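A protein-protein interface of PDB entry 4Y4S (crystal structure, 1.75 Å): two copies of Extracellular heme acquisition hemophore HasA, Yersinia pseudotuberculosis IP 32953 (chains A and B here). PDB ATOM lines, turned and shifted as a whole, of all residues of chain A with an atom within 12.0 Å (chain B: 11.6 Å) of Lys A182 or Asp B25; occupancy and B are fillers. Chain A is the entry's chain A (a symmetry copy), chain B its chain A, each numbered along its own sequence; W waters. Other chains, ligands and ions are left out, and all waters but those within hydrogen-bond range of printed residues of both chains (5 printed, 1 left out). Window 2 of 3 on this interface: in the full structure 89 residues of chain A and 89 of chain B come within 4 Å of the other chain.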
ATOM      1  N   ASP A 125       4.969 -20.151 -25.787  1.00  0.00           N
ATOM      2  CA  ASP A 125       4.868 -21.272 -24.851  1.00  0.00           C
ATOM      3  C   ASP A 125       3.808 -20.966 -23.783  1.00  0.00           C
ATOM      4  O   ASP A 125       2.919 -21.779 -23.527  1.00  0.00           O
ATOM      5  CB  ASP A 125       6.215 -21.592 -24.136  1.00  0.00           C
ATOM      6  CG  ASP A 125       7.360 -21.924 -25.085  1.00  0.00           C
ATOM      7  OD1 ASP A 125       7.132 -22.392 -26.224  1.00  0.00           O
ATOM      8  OD2 ASP A 125       8.519 -21.703 -24.651  1.00  0.00           O
ATOM      9  N   ILE A 126       3.920 -19.809 -23.113  1.00  0.00           N
ATOM     10  CA  ILE A 126       3.040 -19.520 -21.984  1.00  0.00           C
ATOM     11  C   ILE A 126       2.677 -18.039 -22.040  1.00  0.00           C
ATOM     12  O   ILE A 126       3.526 -17.218 -22.350  1.00  0.00           O
ATOM     13  CB  ILE A 126       3.728 -19.880 -20.606  1.00  0.00           C
ATOM     14  CG1 ILE A 126       3.727 -21.406 -20.374  1.00  0.00           C
ATOM     15  CG2 ILE A 126       2.899 -19.401 -19.453  1.00  0.00           C
ATOM     16  CD1 ILE A 126       4.837 -22.079 -20.926  1.00  0.00           C
ATOM     17  N   ASN A 176      -0.078 -19.817  -7.890  1.00  0.00           N
ATOM     18  CA  ASN A 176       0.589 -21.036  -7.482  1.00  0.00           C
ATOM     19  C   ASN A 176       1.595 -21.452  -8.524  1.00  0.00           C
ATOM     20  O   ASN A 176       1.214 -21.871  -9.634  1.00  0.00           O
ATOM     21  CB  ASN A 176      -0.436 -22.139  -7.267  1.00  0.00           C
ATOM     22  CG  ASN A 176       0.186 -23.398  -6.669  1.00  0.00           C
ATOM     23  OD1 ASN A 176       1.130 -23.967  -7.204  1.00  0.00           O
ATOM     24  ND2 ASN A 176      -0.337 -23.814  -5.533  1.00  0.00           N
ATOM     25  N   VAL A 177       2.889 -21.359  -8.193  1.00  0.00           N
ATOM     26  CA  VAL A 177       3.897 -21.647  -9.198  1.00  0.00           C
ATOM     27  C   VAL A 177       4.444 -23.074  -9.160  1.00  0.00           C
ATOM     28  O   VAL A 177       5.349 -23.387  -9.931  1.00  0.00           O
ATOM     29  CB  VAL A 177       5.085 -20.662  -9.093  1.00  0.00           C
ATOM     30  CG1 VAL A 177       4.544 -19.258  -9.147  1.00  0.00           C
ATOM     31  CG2 VAL A 177       5.852 -20.848  -7.757  1.00  0.00           C
ATOM     32  N   ASP A 178       3.946 -23.905  -8.231  1.00  0.00           N
ATOM     33  CA  ASP A 178       4.413 -25.309  -8.078  1.00  0.00           C
ATOM     34  C   ASP A 178       3.389 -26.388  -8.480  1.00  0.00           C
ATOM     35  O   ASP A 178       3.431 -27.515  -7.969  1.00  0.00           O
ATOM     36  CB  ASP A 178       4.825 -25.553  -6.608  1.00  0.00           C
ATOM     37  CG  ASP A 178       5.976 -24.664  -6.182  1.00  0.00           C
ATOM     38  OD1 ASP A 178       7.059 -24.720  -6.814  1.00  0.00           O
ATOM     39  OD2 ASP A 178       5.787 -23.900  -5.218  1.00  0.00           O
ATOM     40  N   THR A 179       2.464 -26.024  -9.363  1.00  0.00           N
ATOM     41  CA  THR A 179       1.375 -26.914  -9.847  1.00  0.00           C
ATOM     42  C   THR A 179       1.526 -27.058 -11.334  1.00  0.00           C
ATOM     43  O   THR A 179       1.748 -26.048 -12.035  1.00  0.00           O
ATOM     44  CB  THR A 179      -0.010 -26.332  -9.562  1.00  0.00           C
ATOM     45  OG1 THR A 179      -0.144 -26.159  -8.152  1.00  0.00           O
ATOM     46  CG2 THR A 179      -1.127 -27.221 -10.103  1.00  0.00           C
ATOM     47  N   ALA A 180       1.447 -28.279 -11.847  1.00  0.00           N
ATOM     48  CA  ALA A 180       1.534 -28.438 -13.283  1.00  0.00           C
ATOM     49  C   ALA A 180       0.403 -27.659 -13.960  1.00  0.00           C
ATOM     50  O   ALA A 180      -0.698 -27.587 -13.420  1.00  0.00           O
ATOM     51  CB  ALA A 180       1.484 -29.934 -13.685  1.00  0.00           C
ATOM     52  N   PHE A 181       0.703 -27.099 -15.133  1.00  0.00           N
ATOM     53  CA  PHE A 181      -0.257 -26.310 -15.909  1.00  0.00           C
ATOM     54  C   PHE A 181      -1.557 -27.082 -16.119  1.00  0.00           C
ATOM     55  O   PHE A 181      -2.620 -26.521 -15.925  1.00  0.00           O
ATOM     56  CB  PHE A 181       0.356 -25.882 -17.268  1.00  0.00           C
ATOM     57  CG  PHE A 181       1.320 -24.758 -17.149  1.00  0.00           C
ATOM     58  CD1 PHE A 181       0.875 -23.500 -16.692  1.00  0.00           C
ATOM     59  CD2 PHE A 181       2.653 -24.940 -17.375  1.00  0.00           C
ATOM     60  CE1 PHE A 181       1.785 -22.453 -16.542  1.00  0.00           C
ATOM     61  CE2 PHE A 181       3.574 -23.865 -17.225  1.00  0.00           C
ATOM     62  CZ  PHE A 181       3.117 -22.649 -16.802  1.00  0.00           C
ATOM     63  N   LYS A 182      -1.463 -28.367 -16.458  1.00  0.00           N
ATOM     64  CA  LYS A 182      -2.661 -29.209 -16.617  1.00  0.00           C
ATOM     65  C   LYS A 182      -3.572 -29.251 -15.391  1.00  0.00           C
ATOM     66  O   LYS A 182      -4.785 -29.383 -15.540  1.00  0.00           O
ATOM     67  CB  LYS A 182      -2.243 -30.632 -17.018  1.00  0.00           C
ATOM     68  CG  LYS A 182      -1.522 -31.449 -15.941  1.00  0.00           C
ATOM     69  CD  LYS A 182      -0.899 -32.672 -16.580  1.00  0.00           C
ATOM     70  CE  LYS A 182      -0.311 -33.605 -15.494  1.00  0.00           C
ATOM     71  NZ  LYS A 182       0.525 -34.725 -16.064  1.00  0.00           N
ATOM     72  N   ASP A 183      -3.006 -29.095 -14.186  1.00  0.00           N
ATOM     73  CA  ASP A 183      -3.770 -29.132 -12.934  1.00  0.00           C
ATOM     74  C   ASP A 183      -3.992 -27.766 -12.374  1.00  0.00           C
ATOM     75  O   ASP A 183      -4.753 -27.570 -11.455  1.00  0.00           O
ATOM     76  CB  ASP A 183      -3.052 -29.999 -11.867  1.00  0.00           C
ATOM     77  CG  ASP A 183      -2.788 -31.408 -12.363  1.00  0.00           C
ATOM     78  OD1 ASP A 183      -3.695 -31.945 -13.018  1.00  0.00           O
ATOM     79  OD2 ASP A 183      -1.667 -31.939 -12.184  1.00  0.00           O
ATOM     80  N   LEU A 184      -3.347 -26.774 -12.947  1.00  0.00           N
ATOM     81  CA  LEU A 184      -3.472 -25.439 -12.393  1.00  0.00           C
ATOM     82  C   LEU A 184      -4.795 -24.799 -12.803  1.00  0.00           C
ATOM     83  O   LEU A 184      -5.076 -24.680 -13.992  1.00  0.00           O
ATOM     84  CB  LEU A 184      -2.304 -24.570 -12.899  1.00  0.00           C
ATOM     85  CG  LEU A 184      -2.147 -23.187 -12.320  1.00  0.00           C
ATOM     86  CD1 LEU A 184      -1.902 -23.130 -10.805  1.00  0.00           C
ATOM     87  CD2 LEU A 184      -0.981 -22.471 -13.089  1.00  0.00           C
ATOM     88  N   SER A 185      -5.557 -24.334 -11.831  1.00  0.00           N
ATOM     89  CA  SER A 185      -6.949 -23.977 -12.062  1.00  0.00           C
ATOM     90  C   SER A 185      -7.102 -22.780 -13.024  1.00  0.00           C
ATOM     91  O   SER A 185      -8.036 -22.756 -13.849  1.00  0.00           O
ATOM     92  CB  SER A 185      -7.623 -23.660 -10.750  1.00  0.00           C
ATOM     93  OG  SER A 185      -8.992 -23.348 -10.984  1.00  0.00           O
ATOM     94  N   ILE A 186      -6.187 -21.805 -12.912  1.00  0.00           N
ATOM     95  CA  ILE A 186      -6.288 -20.557 -13.692  1.00  0.00           C
ATOM     96  C   ILE A 186      -5.654 -20.719 -15.089  1.00  0.00           C
ATOM     97  O   ILE A 186      -5.612 -19.782 -15.907  1.00  0.00           O
ATOM     98  CB  ILE A 186      -5.627 -19.390 -12.935  1.00  0.00           C
ATOM     99  CG1 ILE A 186      -4.120 -19.635 -12.725  1.00  0.00           C
ATOM    100  CG2 ILE A 186      -6.328 -19.150 -11.601  1.00  0.00           C
ATOM    101  CD1 ILE A 186      -3.382 -18.399 -12.277  1.00  0.00           C
ATOM    102  N   ALA A 187      -5.132 -21.908 -15.368  1.00  0.00           N
ATOM    103  CA  ALA A 187      -4.427 -22.132 -16.609  1.00  0.00           C
ATOM    104  C   ALA A 187      -5.339 -22.857 -17.573  1.00  0.00           C
ATOM    105  O   ALA A 187      -6.174 -23.641 -17.136  1.00  0.00           O
ATOM    106  CB  ALA A 187      -3.168 -22.929 -16.363  1.00  0.00           C
ATOM    107  N   SER A 188      -5.197 -22.588 -18.871  1.00  0.00           N
ATOM    108  CA  SER A 188      -5.858 -23.370 -19.878  1.00  0.00           C
ATOM    109  C   SER A 188      -4.921 -23.659 -21.037  1.00  0.00           C
ATOM    110  O   SER A 188      -3.984 -22.896 -21.321  1.00  0.00           O
ATOM    111  CB  SER A 188      -7.119 -22.650 -20.364  1.00  0.00           C
ATOM    112  OG  SER A 188      -6.781 -21.529 -21.188  1.00  0.00           O
ATOM    113  N   GLN A 189      -5.143 -24.768 -21.729  1.00  0.00           N
ATOM    114  CA  GLN A 189      -4.319 -25.120 -22.853  1.00  0.00           C
ATOM    115  C   GLN A 189      -4.756 -24.465 -24.160  1.00  0.00           C
ATOM    116  O   GLN A 189      -5.947 -24.440 -24.470  1.00  0.00           O
ATOM    117  CB  GLN A 189      -4.323 -26.656 -23.019  1.00  0.00           C
ATOM    118  CG  GLN A 189      -3.242 -27.175 -23.917  1.00  0.00           C
ATOM    119  CD  GLN A 189      -3.214 -28.696 -23.966  1.00  0.00           C
ATOM    120  OE1 GLN A 189      -2.675 -29.357 -23.064  1.00  0.00           O
ATOM    121  NE2 GLN A 189      -3.802 -29.258 -25.016  1.00  0.00           N
ATOM    122  N   TYR A 190      -3.793 -23.908 -24.898  1.00  0.00           N
ATOM    123  CA  TYR A 190      -3.998 -23.481 -26.287  1.00  0.00           C
ATOM    124  C   TYR A 190      -4.455 -24.673 -27.130  1.00  0.00           C
ATOM    125  O   TYR A 190      -3.996 -25.789 -26.903  1.00  0.00           O
ATOM    126  CB  TYR A 190      -2.693 -22.926 -26.895  1.00  0.00           C
ATOM    127  CG  TYR A 190      -2.299 -21.503 -26.471  1.00  0.00           C
ATOM    128  CD1 TYR A 190      -3.118 -20.421 -26.759  1.00  0.00           C
ATOM    129  CD2 TYR A 190      -1.064 -21.253 -25.848  1.00  0.00           C
ATOM    130  CE1 TYR A 190      -2.753 -19.123 -26.400  1.00  0.00           C
ATOM    131  CE2 TYR A 190      -0.674 -19.956 -25.510  1.00  0.00           C
ATOM    132  CZ  TYR A 190      -1.519 -18.895 -25.784  1.00  0.00           C
ATOM    133  OH  TYR A 190      -1.144 -17.598 -25.424  1.00  0.00           O
ATOM    134  N   ILE B  17      -3.933 -17.970 -17.337  1.00  0.00           N
ATOM    135  CA  ILE B  17      -2.694 -18.361 -18.002  1.00  0.00           C
ATOM    136  C   ILE B  17      -2.964 -19.329 -19.115  1.00  0.00           C
ATOM    137  O   ILE B  17      -3.804 -20.249 -18.973  1.00  0.00           O
ATOM    138  CB  ILE B  17      -1.719 -19.031 -17.023  1.00  0.00           C
ATOM    139  CG1 ILE B  17      -1.389 -18.049 -15.921  1.00  0.00           C
ATOM    140  CG2 ILE B  17      -0.446 -19.496 -17.745  1.00  0.00           C
ATOM    141  CD1 ILE B  17      -0.668 -18.731 -14.758  1.00  0.00           C
ATOM    142  N   GLN B  18      -2.306 -19.136 -20.243  1.00  0.00           N
ATOM    143  CA  GLN B  18      -2.489 -20.030 -21.367  1.00  0.00           C
ATOM    144  C   GLN B  18      -1.205 -20.743 -21.647  1.00  0.00           C
ATOM    145  O   GLN B  18      -0.158 -20.095 -21.706  1.00  0.00           O
ATOM    146  CB  GLN B  18      -2.949 -19.264 -22.629  1.00  0.00           C
ATOM    147  CG  GLN B  18      -4.306 -18.648 -22.444  1.00  0.00           C
ATOM    148  CD  GLN B  18      -4.705 -17.807 -23.650  1.00  0.00           C
ATOM    149  OE1 GLN B  18      -4.306 -16.667 -23.742  1.00  0.00           O
ATOM    150  NE2 GLN B  18      -5.455 -18.389 -24.592  1.00  0.00           N
ATOM    151  N   TYR B  19      -1.260 -22.051 -21.893  1.00  0.00           N
ATOM    152  CA  TYR B  19      -0.004 -22.743 -22.172  1.00  0.00           C
ATOM    153  C   TYR B  19      -0.051 -23.646 -23.387  1.00  0.00           C
ATOM    154  O   TYR B  19      -1.104 -24.169 -23.724  1.00  0.00           O
ATOM    155  CB  TYR B  19       0.414 -23.559 -20.920  1.00  0.00           C
ATOM    156  CG  TYR B  19      -0.577 -24.668 -20.571  1.00  0.00           C
ATOM    157  CD1 TYR B  19      -1.704 -24.400 -19.807  1.00  0.00           C
ATOM    158  CD2 TYR B  19      -0.391 -25.965 -21.027  1.00  0.00           C
ATOM    159  CE1 TYR B  19      -2.653 -25.449 -19.457  1.00  0.00           C
ATOM    160  CE2 TYR B  19      -1.319 -27.010 -20.679  1.00  0.00           C
ATOM    161  CZ  TYR B  19      -2.428 -26.724 -19.937  1.00  0.00           C
ATOM    162  OH  TYR B  19      -3.313 -27.695 -19.624  1.00  0.00           O
ATOM    163  N   ASN B  20       1.092 -23.819 -24.045  1.00  0.00           N
ATOM    164  CA  ASN B  20       1.181 -24.742 -25.164  1.00  0.00           C
ATOM    165  C   ASN B  20       1.187 -26.195 -24.619  1.00  0.00           C
ATOM    166  O   ASN B  20       1.748 -26.454 -23.567  1.00  0.00           O
ATOM    167  CB  ASN B  20       2.425 -24.441 -25.999  1.00  0.00           C
ATOM    168  CG  ASN B  20       2.604 -25.404 -27.154  1.00  0.00           C
ATOM    169  OD1 ASN B  20       3.106 -26.517 -26.982  1.00  0.00           O
ATOM    170  ND2 ASN B  20       2.177 -24.989 -28.340  1.00  0.00           N
ATOM    171  N   SER B  21       0.518 -27.117 -25.304  1.00  0.00           N
ATOM    172  CA  SER B  21       0.318 -28.465 -24.768  1.00  0.00           C
ATOM    173  C   SER B  21       1.633 -29.171 -24.457  1.00  0.00           C
ATOM    174  O   SER B  21       1.664 -30.088 -23.644  1.00  0.00           O
ATOM    175  CB  SER B  21      -0.502 -29.320 -25.752  1.00  0.00           C
ATOM    176  OG  SER B  21       0.230 -29.534 -26.940  1.00  0.00           O
ATOM    177  N   ASN B  22       2.708 -28.737 -25.085  1.00  0.00           N
ATOM    178  CA  ASN B  22       4.001 -29.323 -24.821  1.00  0.00           C
ATOM    179  C   ASN B  22       4.448 -29.065 -23.382  1.00  0.00           C
ATOM    180  O   ASN B  22       5.299 -29.780 -22.874  1.00  0.00           O
ATOM    181  CB  ASN B  22       5.035 -28.801 -25.813  1.00  0.00           C
ATOM    182  CG  ASN B  22       4.732 -29.231 -27.254  1.00  0.00           C
ATOM    183  OD1 ASN B  22       4.093 -30.262 -27.489  1.00  0.00           O
ATOM    184  ND2 ASN B  22       5.188 -28.435 -28.219  1.00  0.00           N
ATOM    185  N   TYR B  23       3.880 -28.063 -22.720  1.00  0.00           N
ATOM    186  CA  TYR B  23       4.320 -27.767 -21.350  1.00  0.00           C
ATOM    187  C   TYR B  23       3.285 -28.151 -20.297  1.00  0.00           C
ATOM    188  O   TYR B  23       3.351 -27.705 -19.143  1.00  0.00           O
ATOM    189  CB  TYR B  23       4.716 -26.270 -21.250  1.00  0.00           C
ATOM    190  CG  TYR B  23       5.863 -25.974 -22.182  1.00  0.00           C
ATOM    191  CD1 TYR B  23       7.171 -26.193 -21.781  1.00  0.00           C
ATOM    192  CD2 TYR B  23       5.644 -25.546 -23.489  1.00  0.00           C
ATOM    193  CE1 TYR B  23       8.243 -25.980 -22.636  1.00  0.00           C
ATOM    194  CE2 TYR B  23       6.693 -25.324 -24.338  1.00  0.00           C
ATOM    195  CZ  TYR B  23       7.993 -25.541 -23.912  1.00  0.00           C
ATOM    196  OH  TYR B  23       9.058 -25.346 -24.748  1.00  0.00           O
ATOM    197  N   ALA B  24       2.342 -29.020 -20.672  1.00  0.00           N
ATOM    198  CA  ALA B  24       1.248 -29.399 -19.782  1.00  0.00           C
ATOM    199  C   ALA B  24       1.729 -29.968 -18.455  1.00  0.00           C
ATOM    200  O   ALA B  24       1.097 -29.764 -17.422  1.00  0.00           O
ATOM    201  CB  ALA B  24       0.330 -30.425 -20.490  1.00  0.00           C
ATOM    202  N   ASP B  25       2.858 -30.679 -18.474  1.00  0.00           N
ATOM    203  CA  ASP B  25       3.346 -31.299 -17.221  1.00  0.00           C
ATOM    204  C   ASP B  25       4.292 -30.395 -16.416  1.00  0.00           C
ATOM    205  O   ASP B  25       4.702 -30.767 -15.329  1.00  0.00           O
ATOM    206  CB  ASP B  25       4.074 -32.627 -17.504  1.00  0.00           C
ATOM    207  CG  ASP B  25       3.155 -33.713 -18.069  1.00  0.00           C
ATOM    208  OD1 ASP B  25       1.943 -33.679 -17.847  1.00  0.00           O
ATOM    209  OD2 ASP B  25       3.671 -34.619 -18.741  1.00  0.00           O
ATOM    210  N   TYR B  26       4.646 -29.225 -16.953  1.00  0.00           N
ATOM    211  CA  TYR B  26       5.479 -28.240 -16.254  1.00  0.00           C
ATOM    212  C   TYR B  26       4.684 -27.416 -15.259  1.00  0.00           C
ATOM    213  O   TYR B  26       3.486 -27.247 -15.447  1.00  0.00           O
ATOM    214  CB  TYR B  26       6.127 -27.285 -17.282  1.00  0.00           C
ATOM    215  CG  TYR B  26       7.266 -27.826 -18.113  1.00  0.00           C
ATOM    216  CD1 TYR B  26       7.086 -28.838 -19.058  1.00  0.00           C
ATOM    217  CD2 TYR B  26       8.501 -27.256 -18.011  1.00  0.00           C
ATOM    218  CE1 TYR B  26       8.137 -29.280 -19.831  1.00  0.00           C
ATOM    219  CE2 TYR B  26       9.548 -27.677 -18.765  1.00  0.00           C
ATOM    220  CZ  TYR B  26       9.372 -28.683 -19.683  1.00  0.00           C
ATOM    221  OH  TYR B  26      10.475 -29.058 -20.428  1.00  0.00           O
ATOM    222  N   SER B  27       5.326 -26.908 -14.206  1.00  0.00           N
ATOM    223  CA  SER B  27       4.756 -25.832 -13.380  1.00  0.00           C
ATOM    224  C   SER B  27       5.320 -24.495 -13.914  1.00  0.00           C
ATOM    225  O   SER B  27       6.215 -24.471 -14.775  1.00  0.00           O
ATOM    226  CB  SER B  27       5.123 -25.979 -11.901  1.00  0.00           C
ATOM    227  OG  SER B  27       6.548 -26.061 -11.873  1.00  0.00           O
ATOM    228  N   ILE B  28       4.814 -23.391 -13.391  1.00  0.00           N
ATOM    229  CA  ILE B  28       5.365 -22.076 -13.732  1.00  0.00           C
ATOM    230  C   ILE B  28       6.816 -22.054 -13.314  1.00  0.00           C
ATOM    231  O   ILE B  28       7.697 -21.620 -14.056  1.00  0.00           O
ATOM    232  CB  ILE B  28       4.611 -20.979 -12.996  1.00  0.00           C
ATOM    233  CG1 ILE B  28       3.167 -20.891 -13.524  1.00  0.00           C
ATOM    234  CG2 ILE B  28       5.359 -19.609 -13.115  1.00  0.00           C
ATOM    235  CD1 ILE B  28       2.286 -20.028 -12.628  1.00  0.00           C
ATOM    236  N   SER B  29       7.054 -22.582 -12.116  1.00  0.00           N
ATOM    237  CA  SER B  29       8.425 -22.723 -11.618  1.00  0.00           C
ATOM    238  C   SER B  29       9.356 -23.533 -12.511  1.00  0.00           C
ATOM    239  O   SER B  29      10.460 -23.089 -12.810  1.00  0.00           O
ATOM    240  CB  SER B  29       8.398 -23.323 -10.195  1.00  0.00           C
ATOM    241  OG  SER B  29       9.680 -23.239  -9.638  1.00  0.00           O
ATOM    242  N   SER B  30       8.949 -24.725 -12.984  1.00  0.00           N
ATOM    243  CA  SER B  30       9.877 -25.550 -13.736  1.00  0.00           C
ATOM    244  C   SER B  30      10.004 -24.997 -15.171  1.00  0.00           C
ATOM    245  O   SER B  30      11.044 -25.108 -15.777  1.00  0.00           O
ATOM    246  CB  SER B  30       9.446 -27.016 -13.748  1.00  0.00           C
ATOM    247  OG  SER B  30       8.282 -27.250 -14.525  1.00  0.00           O
ATOM    248  N   TYR B  31       8.948 -24.360 -15.679  1.00  0.00           N
ATOM    249  CA  TYR B  31       9.055 -23.718 -16.980  1.00  0.00           C
ATOM    250  C   TYR B  31      10.011 -22.543 -16.931  1.00  0.00           C
ATOM    251  O   TYR B  31      10.837 -22.382 -17.814  1.00  0.00           O
ATOM    252  CB  TYR B  31       7.670 -23.219 -17.521  1.00  0.00           C
ATOM    253  CG  TYR B  31       7.863 -22.504 -18.846  1.00  0.00           C
ATOM    254  CD1 TYR B  31       7.929 -23.216 -20.028  1.00  0.00           C
ATOM    255  CD2 TYR B  31       8.050 -21.119 -18.889  1.00  0.00           C
ATOM    256  CE1 TYR B  31       8.150 -22.557 -21.252  1.00  0.00           C
ATOM    257  CE2 TYR B  31       8.270 -20.459 -20.084  1.00  0.00           C
ATOM    258  CZ  TYR B  31       8.302 -21.159 -21.249  1.00  0.00           C
ATOM    259  OH  TYR B  31       8.552 -20.472 -22.406  1.00  0.00           O
ATOM    260  N   LEU B  32       9.855 -21.672 -15.959  1.00  0.00           N
ATOM    261  CA  LEU B  32      10.661 -20.468 -15.995  1.00  0.00           C
ATOM    262  C   LEU B  32      12.112 -20.839 -15.648  1.00  0.00           C
ATOM    263  O   LEU B  32      13.049 -20.207 -16.161  1.00  0.00           O
ATOM    264  CB  LEU B  32      10.117 -19.405 -15.059  1.00  0.00           C
ATOM    265  CG  LEU B  32       8.872 -18.633 -15.505  1.00  0.00           C
ATOM    266  CD1 LEU B  32       8.468 -17.631 -14.369  1.00  0.00           C
ATOM    267  CD2 LEU B  32       9.112 -17.932 -16.919  1.00  0.00           C
ATOM    268  N   GLU B  34      13.699 -23.602 -16.526  1.00  0.00           N
ATOM    269  CA  GLU B  34      14.204 -24.067 -17.813  1.00  0.00           C
ATOM    270  C   GLU B  34      14.404 -22.917 -18.793  1.00  0.00           C
ATOM    271  O   GLU B  34      15.415 -22.856 -19.447  1.00  0.00           O
ATOM    272  CB  GLU B  34      13.257 -25.085 -18.428  1.00  0.00           C
ATOM    273  CG  GLU B  34      13.762 -25.668 -19.784  1.00  0.00           C
ATOM    274  CD  GLU B  34      12.824 -26.734 -20.357  1.00  0.00           C
ATOM    275  OE1 GLU B  34      12.604 -27.766 -19.679  1.00  0.00           O
ATOM    276  OE2 GLU B  34      12.285 -26.533 -21.468  1.00  0.00           O
HETATM  277  O   HOH W   1       5.235 -23.554 -27.684  1.00  0.00           O
HETATM  278  O   HOH W   2       9.212 -23.133  -7.086  1.00  0.00           O
HETATM  279  O   HOH W   3      -6.315 -19.401 -19.492  1.00  0.00           O
HETATM  280  O   HOH W   4      -1.237 -26.279 -27.413  1.00  0.00           O
HETATM  281  O   HOH W   5      -6.771 -20.961 -23.851  1.00  0.00           O
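No position is printed for both chains.
Of the 39 pairs that touch across the chains among the printed residues, none has its exchanged pair printed and touching as well.
Water W2 lies within hydrogen-bond range of the side-chain hydroxyl of Ser B29 and the side-chain carboxylate of Asp A178.
Water W1 lies within hydrogen-bond range of the side-chain carboxylate (OD1) of Asp A125 (2.7 Å) and the side-chain amide nitrogen (ND2) of Asn B20 (3.4 Å).
Water W3 bridges O of Ile B17 (2.7 Å) and OG of Ser A188 (2.8 Å).
Water W5 bridges OG of Ser A188 (2.7 Å) and NE2 of Gln B18 (3.0 Å).
Water W4 bridges O of Tyr A190 (2.8 Å) and N of Ser B21 (2.9 Å).
Of the 17 printed residues of chain B, 13 touch a printed residue of chain A.
Hydrophobic or aromatic side chains of chain B within 4 Å of the printed part of chain A: Ile B17, Tyr B19, Tyr B23, Ile B28 and Tyr B31.
Of the 17 printed residues of chain A, 14 touch a printed residue of chain B.
Hydrophobic or aromatic side chains of chain A within 4 Å of the printed part of chain B: Ile A126, Val A177, Ala A180, Phe A181, Ile A186, Ala A187 and Tyr A190.
Among the printed residues, 39 pairs touch across the chains.
Among the printed residues, Asp or Glu carboxylates within 4 Å of a Lys or Arg side-chain nitrogen of the other chain: Lys A182 with Asp B25 (2.5 Å).
O of Ile A186 is in hydrogen-bond range of N of Ile B17 (2.9 Å).
The backbone carbonyl oxygen of Tyr B19 is in hydrogen-bond range of the backbone NH of Tyr A190, at 2.9 Å.
The backbone NH of Tyr B19 lies within hydrogen-bond range of the backbone carbonyl oxygen of Ser A188 (2.9 Å).
The backbone NH of Ser B29 lies within hydrogen-bond range of the backbone carbonyl oxygen of Val A177 (2.9 Å).
The backbone NH (N) of Ser A188 lies within hydrogen-bond range of the backbone carbonyl oxygen (O) of Ile B17 (2.7 Å).
OH of Tyr B31 lies within hydrogen-bond range of OD2 of Asp A125 (2.6 Å).
The backbone carbonyl oxygen (O) of Tyr B26 sits at hydrogen-bond distance from the backbone NH (N) of Phe A181 (2.8 Å).
The backbone carbonyl oxygen (O) of Ala B24 sits at hydrogen-bond distance from the backbone NH (N) of Lys A182 (3.1 Å).
N of Asn B20 sits at hydrogen-bond distance from O of Asp A125, at 2.8 Å.
OD1 of Asp B25 is in salt-bridge range of NZ of Lys A182 (2.5 Å).
Of chain B, only Tyr B19, Ala B24 and Asp B25 come within 4 Å of Lys A182.
Of chain A, only Ala A180 and Lys A182 come within 4 Å of Asp B25.
Ala A180 touches three residues of chain B.
Of chain B, only Ile B17, Tyr B19, Tyr B23, Ala B24, Tyr B26, Ser B27 and Ile B28 come within 4 Å of Phe A181.
Of chain B, only Ile B17 comes within 4 Å of Ala A187.
Ala B24 touches three residues of chain A.
Ser B27 touches four residues of chain A.
Of the printed residues of chain A, Ser B21 touches Gln A189 (3.3 Å).
Of the printed residues of chain B, Gln A189 touches Tyr B19 and Ser B21.
Printed residues of chain B within 4 Å of Asp A178: Ser B27 and Ser B29.
Leu A184 touches none of the printed residues of chain B.
Asn B22 touches none of the printed residues of chain A.
The side-chain hydroxyl (OH) of Tyr B26 sits at hydrogen-bond distance from the side-chain carboxylate (OE1) of Glu B34 (2.6 Å).
OD1 of Asn B20 lies within hydrogen-bond range of N of Asn B22, at 2.9 Å.
The backbone NH of Ser B30 sits at hydrogen-bond distance from the side-chain hydroxyl of Ser B27 (3.0 Å).
The side-chain amide oxygen (OD1) of Asn A176 sits at hydrogen-bond distance from the side-chain hydroxyl (OG1) of Thr A179 (2.7 Å).
The side-chain amide oxygen of Asn A176 sits at hydrogen-bond distance from the backbone NH of Asp A178 (3.0 Å).
Among the printed residues, merely in contact across the chains: Asp A125 with Gln B18 (3.95 Å), Asp A125 with Tyr B19 (3.4 Å), Asp A125 with Tyr B23 (3.5 Å), Ile A126 with Ile B17 (3.8 Å), Ile A126 with Gln B18 (3.3 Å), Ile A126 with Tyr B19 (3.99 Å), Ile A126 with Tyr B31 (3.4 Å), Asn A176 with Ile B28 (3.7 Å), Val A177 with Ser B27 (3.3 Å), Val A177 with Ile B28 (3.5 Å), Asp A178 with Ser B27 (3.9 Å), Asp A178 with Ser B29 (3.9 Å), Thr A179 with Ser B27 (3.3 Å), Ala A180 with Ala B24 (3.8 Å), Ala A180 with Asp B25 (3.7 Å), Ala A180 with Tyr B26 (3.1 Å), Phe A181 with Ile B17 (3.9 Å), Phe A181 with Tyr B19 (3.6 Å), Phe A181 with Tyr B23 (3.4 Å), Phe A181 with Ala B24 (3.5 Å), Phe A181 with Ser B27 (3.7 Å), Phe A181 with Ile B28 (3.7 Å), Lys A182 with Tyr B19 (3.4 Å), Ala A187 with Ile B17 (3.1 Å), Ser A188 with Gln B18 (3.2 Å), Gln A189 with Tyr B19 (3.4 Å), Gln A189 with Ser B21 (3.3 Å), Tyr A190 with Gln B18 (3.3 Å) and Tyr A190 with Asn B20 (3.8 Å).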
